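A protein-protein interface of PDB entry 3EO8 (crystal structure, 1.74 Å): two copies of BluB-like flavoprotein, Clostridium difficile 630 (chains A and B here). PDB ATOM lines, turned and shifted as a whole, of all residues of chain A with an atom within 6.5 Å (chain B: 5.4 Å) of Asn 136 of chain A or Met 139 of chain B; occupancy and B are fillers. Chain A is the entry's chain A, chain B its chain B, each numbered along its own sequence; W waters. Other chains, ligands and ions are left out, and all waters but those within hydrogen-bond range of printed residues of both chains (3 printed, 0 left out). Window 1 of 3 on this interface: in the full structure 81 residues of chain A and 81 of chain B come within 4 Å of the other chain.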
ATOM      1  N   ASN A  45     -29.065  14.470 -29.576  1.00  0.00           N
ATOM      2  CA  ASN A  45     -29.858  15.685 -29.467  1.00  0.00           C
ATOM      3  C   ASN A  45     -29.583  16.631 -30.600  1.00  0.00           C
ATOM      4  O   ASN A  45     -28.967  17.690 -30.425  1.00  0.00           O
ATOM      5  CB  ASN A  45     -29.613  16.395 -28.114  1.00  0.00           C
ATOM      6  CG  ASN A  45     -28.119  16.697 -27.831  1.00  0.00           C
ATOM      7  OD1 ASN A  45     -27.207  15.927 -28.225  1.00  0.00           O
ATOM      8  ND2 ASN A  45     -27.869  17.830 -27.152  1.00  0.00           N
ATOM      9  N   VAL A 110     -32.062  20.185 -24.697  1.00  0.00           N
ATOM     10  CA  VAL A 110     -31.310  20.093 -23.454  1.00  0.00           C
ATOM     11  C   VAL A 110     -31.085  18.638 -23.077  1.00  0.00           C
ATOM     12  O   VAL A 110     -31.965  17.801 -23.262  1.00  0.00           O
ATOM     13  CB  VAL A 110     -32.032  20.830 -22.282  1.00  0.00           C
ATOM     14  CG1 VAL A 110     -31.352  20.513 -20.957  1.00  0.00           C
ATOM     15  CG2 VAL A 110     -32.058  22.311 -22.518  1.00  0.00           C
ATOM     16  N   TYR A 111     -29.888  18.332 -22.601  1.00  0.00           N
ATOM     17  CA  TYR A 111     -29.544  17.023 -22.043  1.00  0.00           C
ATOM     18  C   TYR A 111     -29.227  17.223 -20.570  1.00  0.00           C
ATOM     19  O   TYR A 111     -28.308  17.954 -20.236  1.00  0.00           O
ATOM     20  CB  TYR A 111     -28.344  16.426 -22.761  1.00  0.00           C
ATOM     21  CG  TYR A 111     -27.799  15.203 -22.093  1.00  0.00           C
ATOM     22  CD1 TYR A 111     -28.582  14.067 -21.949  1.00  0.00           C
ATOM     23  CD2 TYR A 111     -26.503  15.162 -21.603  1.00  0.00           C
ATOM     24  CE1 TYR A 111     -28.086  12.940 -21.326  1.00  0.00           C
ATOM     25  CE2 TYR A 111     -26.011  14.040 -21.010  1.00  0.00           C
ATOM     26  CZ  TYR A 111     -26.824  12.925 -20.863  1.00  0.00           C
ATOM     27  OH  TYR A 111     -26.329  11.802 -20.236  1.00  0.00           O
ATOM     28  N   PRO A 113     -27.530  15.918 -17.578  1.00  0.00           N
ATOM     29  CA  PRO A 113     -26.432  14.949 -17.514  1.00  0.00           C
ATOM     30  C   PRO A 113     -26.442  14.152 -16.214  1.00  0.00           C
ATOM     31  O   PRO A 113     -27.268  14.407 -15.356  1.00  0.00           O
ATOM     32  CB  PRO A 113     -25.185  15.844 -17.591  1.00  0.00           C
ATOM     33  CG  PRO A 113     -25.639  17.129 -16.893  1.00  0.00           C
ATOM     34  CD  PRO A 113     -27.089  17.283 -17.229  1.00  0.00           C
ATOM     35  N   LYS A 131     -23.676  23.589 -11.663  1.00  0.00           N
ATOM     36  CA  LYS A 131     -22.272  23.300 -11.982  1.00  0.00           C
ATOM     37  C   LYS A 131     -22.104  22.190 -13.013  1.00  0.00           C
ATOM     38  O   LYS A 131     -21.129  22.204 -13.766  1.00  0.00           O
ATOM     39  CB  LYS A 131     -21.491  22.951 -10.729  1.00  0.00           C
ATOM     40  CG  LYS A 131     -21.463  24.120  -9.716  1.00  0.00           C
ATOM     41  CD  LYS A 131     -20.663  23.817  -8.471  1.00  0.00           C
ATOM     42  CE  LYS A 131     -20.715  25.005  -7.513  1.00  0.00           C
ATOM     43  NZ  LYS A 131     -20.023  24.690  -6.220  1.00  0.00           N
ATOM     44  N   LEU A 132     -23.048  21.248 -13.093  1.00  0.00           N
ATOM     45  CA  LEU A 132     -22.976  20.226 -14.155  1.00  0.00           C
ATOM     46  C   LEU A 132     -23.031  20.857 -15.539  1.00  0.00           C
ATOM     47  O   LEU A 132     -22.474  20.315 -16.504  1.00  0.00           O
ATOM     48  CB  LEU A 132     -24.093  19.170 -13.998  1.00  0.00           C
ATOM     49  CG  LEU A 132     -24.122  18.453 -12.627  1.00  0.00           C
ATOM     50  CD1 LEU A 132     -25.404  17.658 -12.417  1.00  0.00           C
ATOM     51  CD2 LEU A 132     -22.857  17.579 -12.483  1.00  0.00           C
ATOM     52  N   PHE A 133     -23.714  22.004 -15.650  1.00  0.00           N
ATOM     53  CA  PHE A 133     -23.961  22.593 -16.946  1.00  0.00           C
ATOM     54  C   PHE A 133     -22.872  23.544 -17.446  1.00  0.00           C
ATOM     55  O   PHE A 133     -22.868  23.877 -18.638  1.00  0.00           O
ATOM     56  CB  PHE A 133     -25.314  23.286 -16.966  1.00  0.00           C
ATOM     57  CG  PHE A 133     -26.473  22.339 -16.898  1.00  0.00           C
ATOM     58  CD1 PHE A 133     -26.947  21.733 -18.040  1.00  0.00           C
ATOM     59  CD2 PHE A 133     -27.123  22.090 -15.688  1.00  0.00           C
ATOM     60  CE1 PHE A 133     -28.008  20.866 -17.997  1.00  0.00           C
ATOM     61  CE2 PHE A 133     -28.202  21.215 -15.636  1.00  0.00           C
ATOM     62  CZ  PHE A 133     -28.634  20.603 -16.807  1.00  0.00           C
ATOM     63  N   ILE A 134     -21.931  23.946 -16.583  1.00  0.00           N
ATOM     64  CA  ILE A 134     -20.797  24.768 -17.049  1.00  0.00           C
ATOM     65  C   ILE A 134     -19.943  24.007 -18.089  1.00  0.00           C
ATOM     66  O   ILE A 134     -19.193  24.616 -18.833  1.00  0.00           O
ATOM     67  CB  ILE A 134     -19.921  25.340 -15.893  1.00  0.00           C
ATOM     68  CG1 ILE A 134     -19.104  24.259 -15.185  1.00  0.00           C
ATOM     69  CG2 ILE A 134     -20.750  26.124 -14.915  1.00  0.00           C
ATOM     70  CD1 ILE A 134     -18.033  24.877 -14.234  1.00  0.00           C
ATOM     71  N   ARG A 135     -20.035  22.677 -18.091  1.00  0.00           N
ATOM     72  CA  ARG A 135     -19.381  21.860 -19.106  1.00  0.00           C
ATOM     73  C   ARG A 135     -20.418  21.155 -19.972  1.00  0.00           C
ATOM     74  O   ARG A 135     -20.084  20.220 -20.685  1.00  0.00           O
ATOM     75  CB  ARG A 135     -18.417  20.862 -18.454  1.00  0.00           C
ATOM     76  CG  ARG A 135     -19.038  19.888 -17.522  1.00  0.00           C
ATOM     77  CD  ARG A 135     -19.063  20.369 -16.081  1.00  0.00           C
ATOM     78  NE  ARG A 135     -17.719  20.514 -15.550  1.00  0.00           N
ATOM     79  CZ  ARG A 135     -17.423  20.952 -14.333  1.00  0.00           C
ATOM     80  NH1 ARG A 135     -18.380  21.259 -13.459  1.00  0.00           N
ATOM     81  NH2 ARG A 135     -16.152  21.030 -13.941  1.00  0.00           N
ATOM     82  N   ASN A 136     -21.636  21.699 -19.981  1.00  0.00           N
ATOM     83  CA  ASN A 136     -22.757  21.213 -20.808  1.00  0.00           C
ATOM     84  C   ASN A 136     -22.471  19.997 -21.719  1.00  0.00           C
ATOM     85  O   ASN A 136     -22.157  20.148 -22.904  1.00  0.00           O
ATOM     86  CB  ASN A 136     -23.320  22.371 -21.646  1.00  0.00           C
ATOM     87  CG  ASN A 136     -24.767  22.204 -21.945  1.00  0.00           C
ATOM     88  OD1 ASN A 136     -25.196  21.135 -22.393  1.00  0.00           O
ATOM     89  ND2 ASN A 136     -25.554  23.226 -21.646  1.00  0.00           N
ATOM     90  N   PRO A 137     -22.565  18.771 -21.153  1.00  0.00           N
ATOM     91  CA  PRO A 137     -22.385  17.553 -21.957  1.00  0.00           C
ATOM     92  C   PRO A 137     -23.310  17.453 -23.189  1.00  0.00           C
ATOM     93  O   PRO A 137     -22.901  16.952 -24.245  1.00  0.00           O
ATOM     94  CB  PRO A 137     -22.557  16.434 -20.921  1.00  0.00           C
ATOM     95  CG  PRO A 137     -22.100  17.077 -19.614  1.00  0.00           C
ATOM     96  CD  PRO A 137     -22.733  18.455 -19.722  1.00  0.00           C
ATOM     97  N   GLY A 138     -24.525  17.998 -23.107  1.00  0.00           N
ATOM     98  CA  GLY A 138     -25.399  18.055 -24.294  1.00  0.00           C
ATOM     99  C   GLY A 138     -24.786  18.806 -25.464  1.00  0.00           C
ATOM    100  O   GLY A 138     -24.945  18.432 -26.633  1.00  0.00           O
ATOM    101  N   MET A 139     -24.096  19.879 -25.151  1.00  0.00           N
ATOM    102  CA  MET A 139     -23.500  20.698 -26.156  1.00  0.00           C
ATOM    103  C   MET A 139     -22.161  20.174 -26.587  1.00  0.00           C
ATOM    104  O   MET A 139     -21.776  20.354 -27.758  1.00  0.00           O
ATOM    105  CB  MET A 139     -23.459  22.152 -25.730  1.00  0.00           C
ATOM    106  CG  MET A 139     -24.854  22.701 -25.540  1.00  0.00           C
ATOM    107  SD  MET A 139     -26.053  22.505 -27.096  1.00  0.00           S
ATOM    108  CE  MET A 139     -27.459  21.556 -26.192  1.00  0.00           C
ATOM    109  N   GLN A 140     -21.468  19.465 -25.689  1.00  0.00           N
ATOM    110  CA  GLN A 140     -20.327  18.708 -26.143  1.00  0.00           C
ATOM    111  C   GLN A 140     -20.767  17.694 -27.195  1.00  0.00           C
ATOM    112  O   GLN A 140     -20.097  17.494 -28.211  1.00  0.00           O
ATOM    113  CB  GLN A 140     -19.651  17.984 -24.988  1.00  0.00           C
ATOM    114  CG  GLN A 140     -18.986  18.849 -23.948  1.00  0.00           C
ATOM    115  CD  GLN A 140     -18.141  18.034 -22.992  1.00  0.00           C
ATOM    116  OE1 GLN A 140     -17.418  17.165 -23.408  1.00  0.00           O
ATOM    117  NE2 GLN A 140     -18.240  18.321 -21.704  1.00  0.00           N
ATOM    118  N   SER A 141     -21.898  17.030 -26.943  1.00  0.00           N
ATOM    119  CA  SER A 141     -22.457  16.050 -27.873  1.00  0.00           C
ATOM    120  C   SER A 141     -22.796  16.712 -29.209  1.00  0.00           C
ATOM    121  O   SER A 141     -22.456  16.190 -30.288  1.00  0.00           O
ATOM    122  CB  SER A 141     -23.713  15.390 -27.290  1.00  0.00           C
ATOM    123  OG  SER A 141     -23.452  14.752 -26.026  1.00  0.00           O
ATOM    124  N   GLY A 143     -21.519  19.390 -30.524  1.00  0.00           N
ATOM    125  CA  GLY A 143     -20.246  19.694 -31.182  1.00  0.00           C
ATOM    126  C   GLY A 143     -19.617  18.509 -31.869  1.00  0.00           C
ATOM    127  O   GLY A 143     -19.072  18.626 -32.997  1.00  0.00           O
ATOM    128  N   ALA A 144     -19.698  17.348 -31.229  1.00  0.00           N
ATOM    129  CA  ALA A 144     -19.212  16.114 -31.847  1.00  0.00           C
ATOM    130  C   ALA A 144     -19.948  15.840 -33.164  1.00  0.00           C
ATOM    131  O   ALA A 144     -19.323  15.541 -34.194  1.00  0.00           O
ATOM    132  CB  ALA A 144     -19.342  14.942 -30.874  1.00  0.00           C
ATOM    133  N   ASN B  45     -10.539  26.539 -26.182  1.00  0.00           N
ATOM    134  CA  ASN B  45     -10.766  26.370 -24.740  1.00  0.00           C
ATOM    135  C   ASN B  45     -10.600  24.928 -24.308  1.00  0.00           C
ATOM    136  O   ASN B  45     -11.561  24.250 -23.925  1.00  0.00           O
ATOM    137  CB  ASN B  45     -12.131  26.914 -24.314  1.00  0.00           C
ATOM    138  CG  ASN B  45     -13.313  26.301 -25.100  1.00  0.00           C
ATOM    139  OD1 ASN B  45     -13.211  25.999 -26.293  1.00  0.00           O
ATOM    140  ND2 ASN B  45     -14.457  26.147 -24.418  1.00  0.00           N
ATOM    141  N   THR B 108     -11.247  22.615 -19.671  1.00  0.00           N
ATOM    142  CA  THR B 108     -11.856  23.601 -20.545  1.00  0.00           C
ATOM    143  C   THR B 108     -12.064  24.884 -19.731  1.00  0.00           C
ATOM    144  O   THR B 108     -11.751  24.939 -18.532  1.00  0.00           O
ATOM    145  CB  THR B 108     -13.163  23.036 -21.126  1.00  0.00           C
ATOM    146  OG1 THR B 108     -13.628  23.853 -22.205  1.00  0.00           O
ATOM    147  CG2 THR B 108     -14.267  22.878 -20.030  1.00  0.00           C
ATOM    148  N   LYS B 109     -12.573  25.916 -20.388  1.00  0.00           N
ATOM    149  CA  LYS B 109     -12.921  27.164 -19.721  1.00  0.00           C
ATOM    150  C   LYS B 109     -14.197  27.729 -20.338  1.00  0.00           C
ATOM    151  O   LYS B 109     -14.590  27.339 -21.427  1.00  0.00           O
ATOM    152  CB  LYS B 109     -11.778  28.179 -19.765  1.00  0.00           C
ATOM    153  CG  LYS B 109     -11.311  28.564 -21.109  1.00  0.00           C
ATOM    154  CD  LYS B 109     -10.310  29.716 -21.058  1.00  0.00           C
ATOM    155  CE  LYS B 109      -9.773  30.040 -22.429  1.00  0.00           C
ATOM    156  NZ  LYS B 109      -8.796  31.199 -22.429  1.00  0.00           N
ATOM    157  N   VAL B 110     -14.876  28.591 -19.602  1.00  0.00           N
ATOM    158  CA  VAL B 110     -16.096  29.211 -20.098  1.00  0.00           C
ATOM    159  C   VAL B 110     -15.767  30.100 -21.297  1.00  0.00           C
ATOM    160  O   VAL B 110     -14.762  30.823 -21.272  1.00  0.00           O
ATOM    161  CB  VAL B 110     -16.780  30.052 -19.000  1.00  0.00           C
ATOM    162  CG1 VAL B 110     -17.961  30.890 -19.553  1.00  0.00           C
ATOM    163  CG2 VAL B 110     -17.281  29.174 -17.856  1.00  0.00           C
ATOM    164  N   PHE B 133     -26.418  30.634 -23.387  1.00  0.00           N
ATOM    165  CA  PHE B 133     -25.715  29.441 -22.854  1.00  0.00           C
ATOM    166  C   PHE B 133     -26.504  28.143 -22.905  1.00  0.00           C
ATOM    167  O   PHE B 133     -25.911  27.094 -22.721  1.00  0.00           O
ATOM    168  CB  PHE B 133     -25.246  29.686 -21.427  1.00  0.00           C
ATOM    169  CG  PHE B 133     -24.179  30.736 -21.317  1.00  0.00           C
ATOM    170  CD1 PHE B 133     -22.847  30.403 -21.528  1.00  0.00           C
ATOM    171  CD2 PHE B 133     -24.497  32.041 -21.026  1.00  0.00           C
ATOM    172  CE1 PHE B 133     -21.837  31.367 -21.437  1.00  0.00           C
ATOM    173  CE2 PHE B 133     -23.482  33.023 -20.938  1.00  0.00           C
ATOM    174  CZ  PHE B 133     -22.150  32.660 -21.157  1.00  0.00           C
ATOM    175  N   ILE B 134     -27.799  28.178 -23.233  1.00  0.00           N
ATOM    176  CA  ILE B 134     -28.549  26.916 -23.355  1.00  0.00           C
ATOM    177  C   ILE B 134     -27.989  26.082 -24.531  1.00  0.00           C
ATOM    178  O   ILE B 134     -28.190  24.858 -24.591  1.00  0.00           O
ATOM    179  CB  ILE B 134     -30.105  27.119 -23.432  1.00  0.00           C
ATOM    180  CG1 ILE B 134     -30.529  27.802 -24.744  1.00  0.00           C
ATOM    181  CG2 ILE B 134     -30.637  27.898 -22.156  1.00  0.00           C
ATOM    182  CD1 ILE B 134     -32.016  27.614 -25.019  1.00  0.00           C
ATOM    183  N   ASN B 136     -24.649  26.532 -25.291  1.00  0.00           N
ATOM    184  CA  ASN B 136     -23.233  26.676 -24.910  1.00  0.00           C
ATOM    185  C   ASN B 136     -22.219  26.468 -26.028  1.00  0.00           C
ATOM    186  O   ASN B 136     -21.681  25.357 -26.198  1.00  0.00           O
ATOM    187  CB  ASN B 136     -22.917  25.741 -23.727  1.00  0.00           C
ATOM    188  CG  ASN B 136     -21.731  26.217 -22.921  1.00  0.00           C
ATOM    189  OD1 ASN B 136     -20.672  26.588 -23.487  1.00  0.00           O
ATOM    190  ND2 ASN B 136     -21.916  26.294 -21.600  1.00  0.00           N
ATOM    191  N   PRO B 137     -21.950  27.544 -26.798  1.00  0.00           N
ATOM    192  CA  PRO B 137     -20.958  27.439 -27.891  1.00  0.00           C
ATOM    193  C   PRO B 137     -19.569  27.022 -27.409  1.00  0.00           C
ATOM    194  O   PRO B 137     -18.846  26.380 -28.154  1.00  0.00           O
ATOM    195  CB  PRO B 137     -20.949  28.854 -28.484  1.00  0.00           C
ATOM    196  CG  PRO B 137     -22.338  29.371 -28.214  1.00  0.00           C
ATOM    197  CD  PRO B 137     -22.615  28.858 -26.807  1.00  0.00           C
ATOM    198  N   GLY B 138     -19.217  27.364 -26.175  1.00  0.00           N
ATOM    199  CA  GLY B 138     -17.928  26.926 -25.610  1.00  0.00           C
ATOM    200  C   GLY B 138     -17.822  25.416 -25.517  1.00  0.00           C
ATOM    201  O   GLY B 138     -16.760  24.827 -25.745  1.00  0.00           O
ATOM    202  N   MET B 139     -18.933  24.764 -25.196  1.00  0.00           N
ATOM    203  CA  MET B 139     -18.917  23.309 -25.095  1.00  0.00           C
ATOM    204  C   MET B 139     -19.120  22.646 -26.439  1.00  0.00           C
ATOM    205  O   MET B 139     -18.650  21.554 -26.634  1.00  0.00           O
ATOM    206  CB  MET B 139     -19.912  22.817 -24.065  1.00  0.00           C
ATOM    207  CG  MET B 139     -19.574  23.264 -22.657  1.00  0.00           C
ATOM    208  SD  MET B 139     -17.685  22.878 -22.142  1.00  0.00           S
ATOM    209  CE  MET B 139     -16.902  24.623 -21.938  1.00  0.00           C
ATOM    210  N   GLN B 140     -19.795  23.307 -27.381  1.00  0.00           N
ATOM    211  CA  GLN B 140     -19.735  22.833 -28.781  1.00  0.00           C
ATOM    212  C   GLN B 140     -18.315  22.769 -29.261  1.00  0.00           C
ATOM    213  O   GLN B 140     -17.891  21.763 -29.901  1.00  0.00           O
ATOM    214  CB  GLN B 140     -20.566  23.747 -29.696  1.00  0.00           C
ATOM    215  CG  GLN B 140     -22.061  23.710 -29.433  1.00  0.00           C
ATOM    216  CD  GLN B 140     -22.861  24.424 -30.514  1.00  0.00           C
ATOM    217  OE1 GLN B 140     -22.627  24.216 -31.677  1.00  0.00           O
ATOM    218  NE2 GLN B 140     -23.824  25.262 -30.110  1.00  0.00           N
ATOM    219  N   SER B 141     -17.550  23.821 -28.964  1.00  0.00           N
ATOM    220  CA  SER B 141     -16.153  23.888 -29.355  1.00  0.00           C
ATOM    221  C   SER B 141     -15.383  22.748 -28.710  1.00  0.00           C
ATOM    222  O   SER B 141     -14.643  22.052 -29.375  1.00  0.00           O
ATOM    223  CB  SER B 141     -15.525  25.236 -28.951  1.00  0.00           C
ATOM    224  OG  SER B 141     -16.322  26.329 -29.362  1.00  0.00           O
ATOM    225  N   LEU B 142     -15.537  22.564 -27.406  1.00  0.00           N
ATOM    226  CA  LEU B 142     -14.830  21.461 -26.749  1.00  0.00           C
ATOM    227  C   LEU B 142     -15.185  20.135 -27.431  1.00  0.00           C
ATOM    228  O   LEU B 142     -14.346  19.283 -27.626  1.00  0.00           O
ATOM    229  CB  LEU B 142     -15.178  21.398 -25.265  1.00  0.00           C
ATOM    230  CG  LEU B 142     -14.376  20.349 -24.486  1.00  0.00           C
ATOM    231  CD1 LEU B 142     -12.915  20.754 -24.555  1.00  0.00           C
ATOM    232  CD2 LEU B 142     -14.858  20.197 -23.052  1.00  0.00           C
ATOM    233  N   GLY B 143     -16.466  19.929 -27.739  1.00  0.00           N
ATOM    234  CA  GLY B 143     -16.880  18.677 -28.369  1.00  0.00           C
ATOM    235  C   GLY B 143     -16.268  18.438 -29.742  1.00  0.00           C
ATOM    236  O   GLY B 143     -15.961  17.300 -30.093  1.00  0.00           O
ATOM    237  N   ALA B 144     -16.060  19.509 -30.512  1.00  0.00           N
ATOM    238  CA  ALA B 144     -15.365  19.410 -31.816  1.00  0.00           C
ATOM    239  C   ALA B 144     -13.929  18.896 -31.591  1.00  0.00           C
ATOM    240  O   ALA B 144     -13.435  18.044 -32.349  1.00  0.00           O
ATOM    241  CB  ALA B 144     -15.359  20.804 -32.559  1.00  0.00           C
ATOM    242  N   PHE B 189     -11.407  24.235 -15.840  1.00  0.00           N
ATOM    243  CA  PHE B 189     -12.041  23.219 -15.001  1.00  0.00           C
ATOM    244  C   PHE B 189     -12.211  21.936 -15.840  1.00  0.00           C
ATOM    245  O   PHE B 189     -12.106  21.964 -17.037  1.00  0.00           O
ATOM    246  CB  PHE B 189     -13.396  23.687 -14.482  1.00  0.00           C
ATOM    247  CG  PHE B 189     -14.286  24.302 -15.536  1.00  0.00           C
ATOM    248  CD1 PHE B 189     -15.135  23.511 -16.320  1.00  0.00           C
ATOM    249  CD2 PHE B 189     -14.267  25.666 -15.765  1.00  0.00           C
ATOM    250  CE1 PHE B 189     -15.949  24.085 -17.280  1.00  0.00           C
ATOM    251  CE2 PHE B 189     -15.097  26.237 -16.713  1.00  0.00           C
ATOM    252  CZ  PHE B 189     -15.930  25.446 -17.476  1.00  0.00           C
HETATM  253  O   HOH W   1     -19.745  27.143 -19.772  1.00  0.00           O
HETATM  254  O   HOH W   2     -24.593  25.708 -20.416  1.00  0.00           O
HETATM  255  O   HOH W   3     -28.466  23.236 -22.346  1.00  0.00           O
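N of Gly 138 of chain B sits close to OD1 of Asn 136 of chain B (3.2 Å).
The backbone carbonyl oxygen of Arg 135 of chain A lies within hydrogen-bond range of the side-chain amide nitrogen of Gln 140 of chain A (2.8 Å).
N of Gly 138 of chain A lies close to OD1 of Asn 136 of chain A.
The side-chain amide oxygen (OD1) of Asn 136 of chain A sits at hydrogen-bond distance from the backbone NH (N) of Met 139 of chain A (3.2 Å).
The backbone NH (N) of Met 139 of chain B lies within hydrogen-bond range of the side-chain amide oxygen (OD1) of Asn 136 of chain B, 3.0 Å away.
NH1 of Arg 135 of chain A sits at hydrogen-bond distance from O of Lys 131 of chain A (2.9 Å).
Water W1 bridges the backbone carbonyl oxygen (O) of Ile 134 of chain A (2.8 Å) and the side-chain amide nitrogen (ND2) of Asn 136 of chain B (3.0 Å).
Water W3 lies within hydrogen-bond range of O of Ile 134 of chain B and ND2 of Asn 136 of chain A.
Water W2 lies within hydrogen-bond range of ND2 of Asn 136 of chain A (2.9 Å), ND2 of Asn 136 of chain B (3.0 Å), O of Phe 133 of chain B (3.0 Å) and O of Phe 133 of chain A (3.1 Å).
Phe 133 of chain A touches Asn 136 of chain B, but with the chains exchanged Asn 136 of chain A does not touch Phe 133 of chain B (4.03 Å).
Asn 136 of chain A touches its own counterpart, Asn 136 of chain B.
Met 139 of chain A touches Gln 140 of chain B, and with the chains exchanged Gln 140 of chain A touches Met 139 of chain B.
Gln 140 of chain A touches Gly 143 of chain B, and with the chains exchanged Gly 143 of chain A touches Gln 140 of chain B.
Positions printed for both chains: 45, 110, 133, 134, 136, 137, 138, 139, 140, 141, 143 and 144.
Among the printed residues, merely in contact across the chains: Phe 133 of chain A with Asn 136 of chain B (3.9 Å), Ile 134 of chain A with Met 139 of chain B (3.9 Å), Ile 134 of chain A with Phe 189 of chain B (3.6 Å), Arg 135 of chain A with Met 139 of chain B (3.5 Å), Arg 135 of chain A with Phe 189 of chain B (3.6 Å), Asn 136 of chain A with Asn 136 of chain B (3.98 Å), Asn 136 of chain A with Met 139 of chain B (3.7 Å), Met 139 of chain A with Ile 134 of chain B (3.7 Å), Met 139 of chain A with Asn 136 of chain B (3.7 Å), Met 139 of chain A with Met 139 of chain B (3.5 Å), Met 139 of chain A with Gln 140 of chain B (3.4 Å), Gln 140 of chain A with Met 139 of chain B (3.3 Å), Gln 140 of chain A with Leu 142 of chain B (3.9 Å), Gln 140 of chain A with Gly 143 of chain B (3.4 Å), Gly 143 of chain A with Gln 140 of chain B (3.4 Å), Gly 143 of chain A with Gly 143 of chain B (3.97 Å), Gly 143 of chain A with Ala 144 of chain B (3.9 Å) and Ala 144 of chain A with Gly 143 of chain B (3.9 Å).
Val 110 of chain A touches none of the printed residues of chain B.
Of the printed residues of chain B, Ile 134 of chain A touches Met 139 and Phe 189.
Of the printed residues of chain B, Asn 136 of chain A touches Asn 136 (3.98 Å) and Met 139 (3.7 Å).
Of the printed residues of chain B, Gln 140 of chain A touches Met 139, Leu 142 and Gly 143.
Val 110 of chain B touches none of the printed residues of chain A.
Of the printed residues of chain A, Met 139 of chain B touches Ile 134 (3.9 Å), Arg 135 (3.5 Å), Asn 136 (3.7 Å), Met 139 (3.5 Å) and Gln 140 (3.3 Å).
The nearest residue of chain A that does not touch Met 139 of chain B is Gly 143 of chain A (5.2 Å).
The nearest printed residue of chain B that does not touch Gln 140 of chain A is Gln 140 of chain B (4.5 Å).
Of the 17 printed residues of chain A, 8 touch a printed residue of chain B.
Hydrophobic or aromatic side chains of chain A within 4 Å of the printed part of chain B: Ile 134 and Met 139.
Among the printed residues, 18 pairs touch across the chains.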
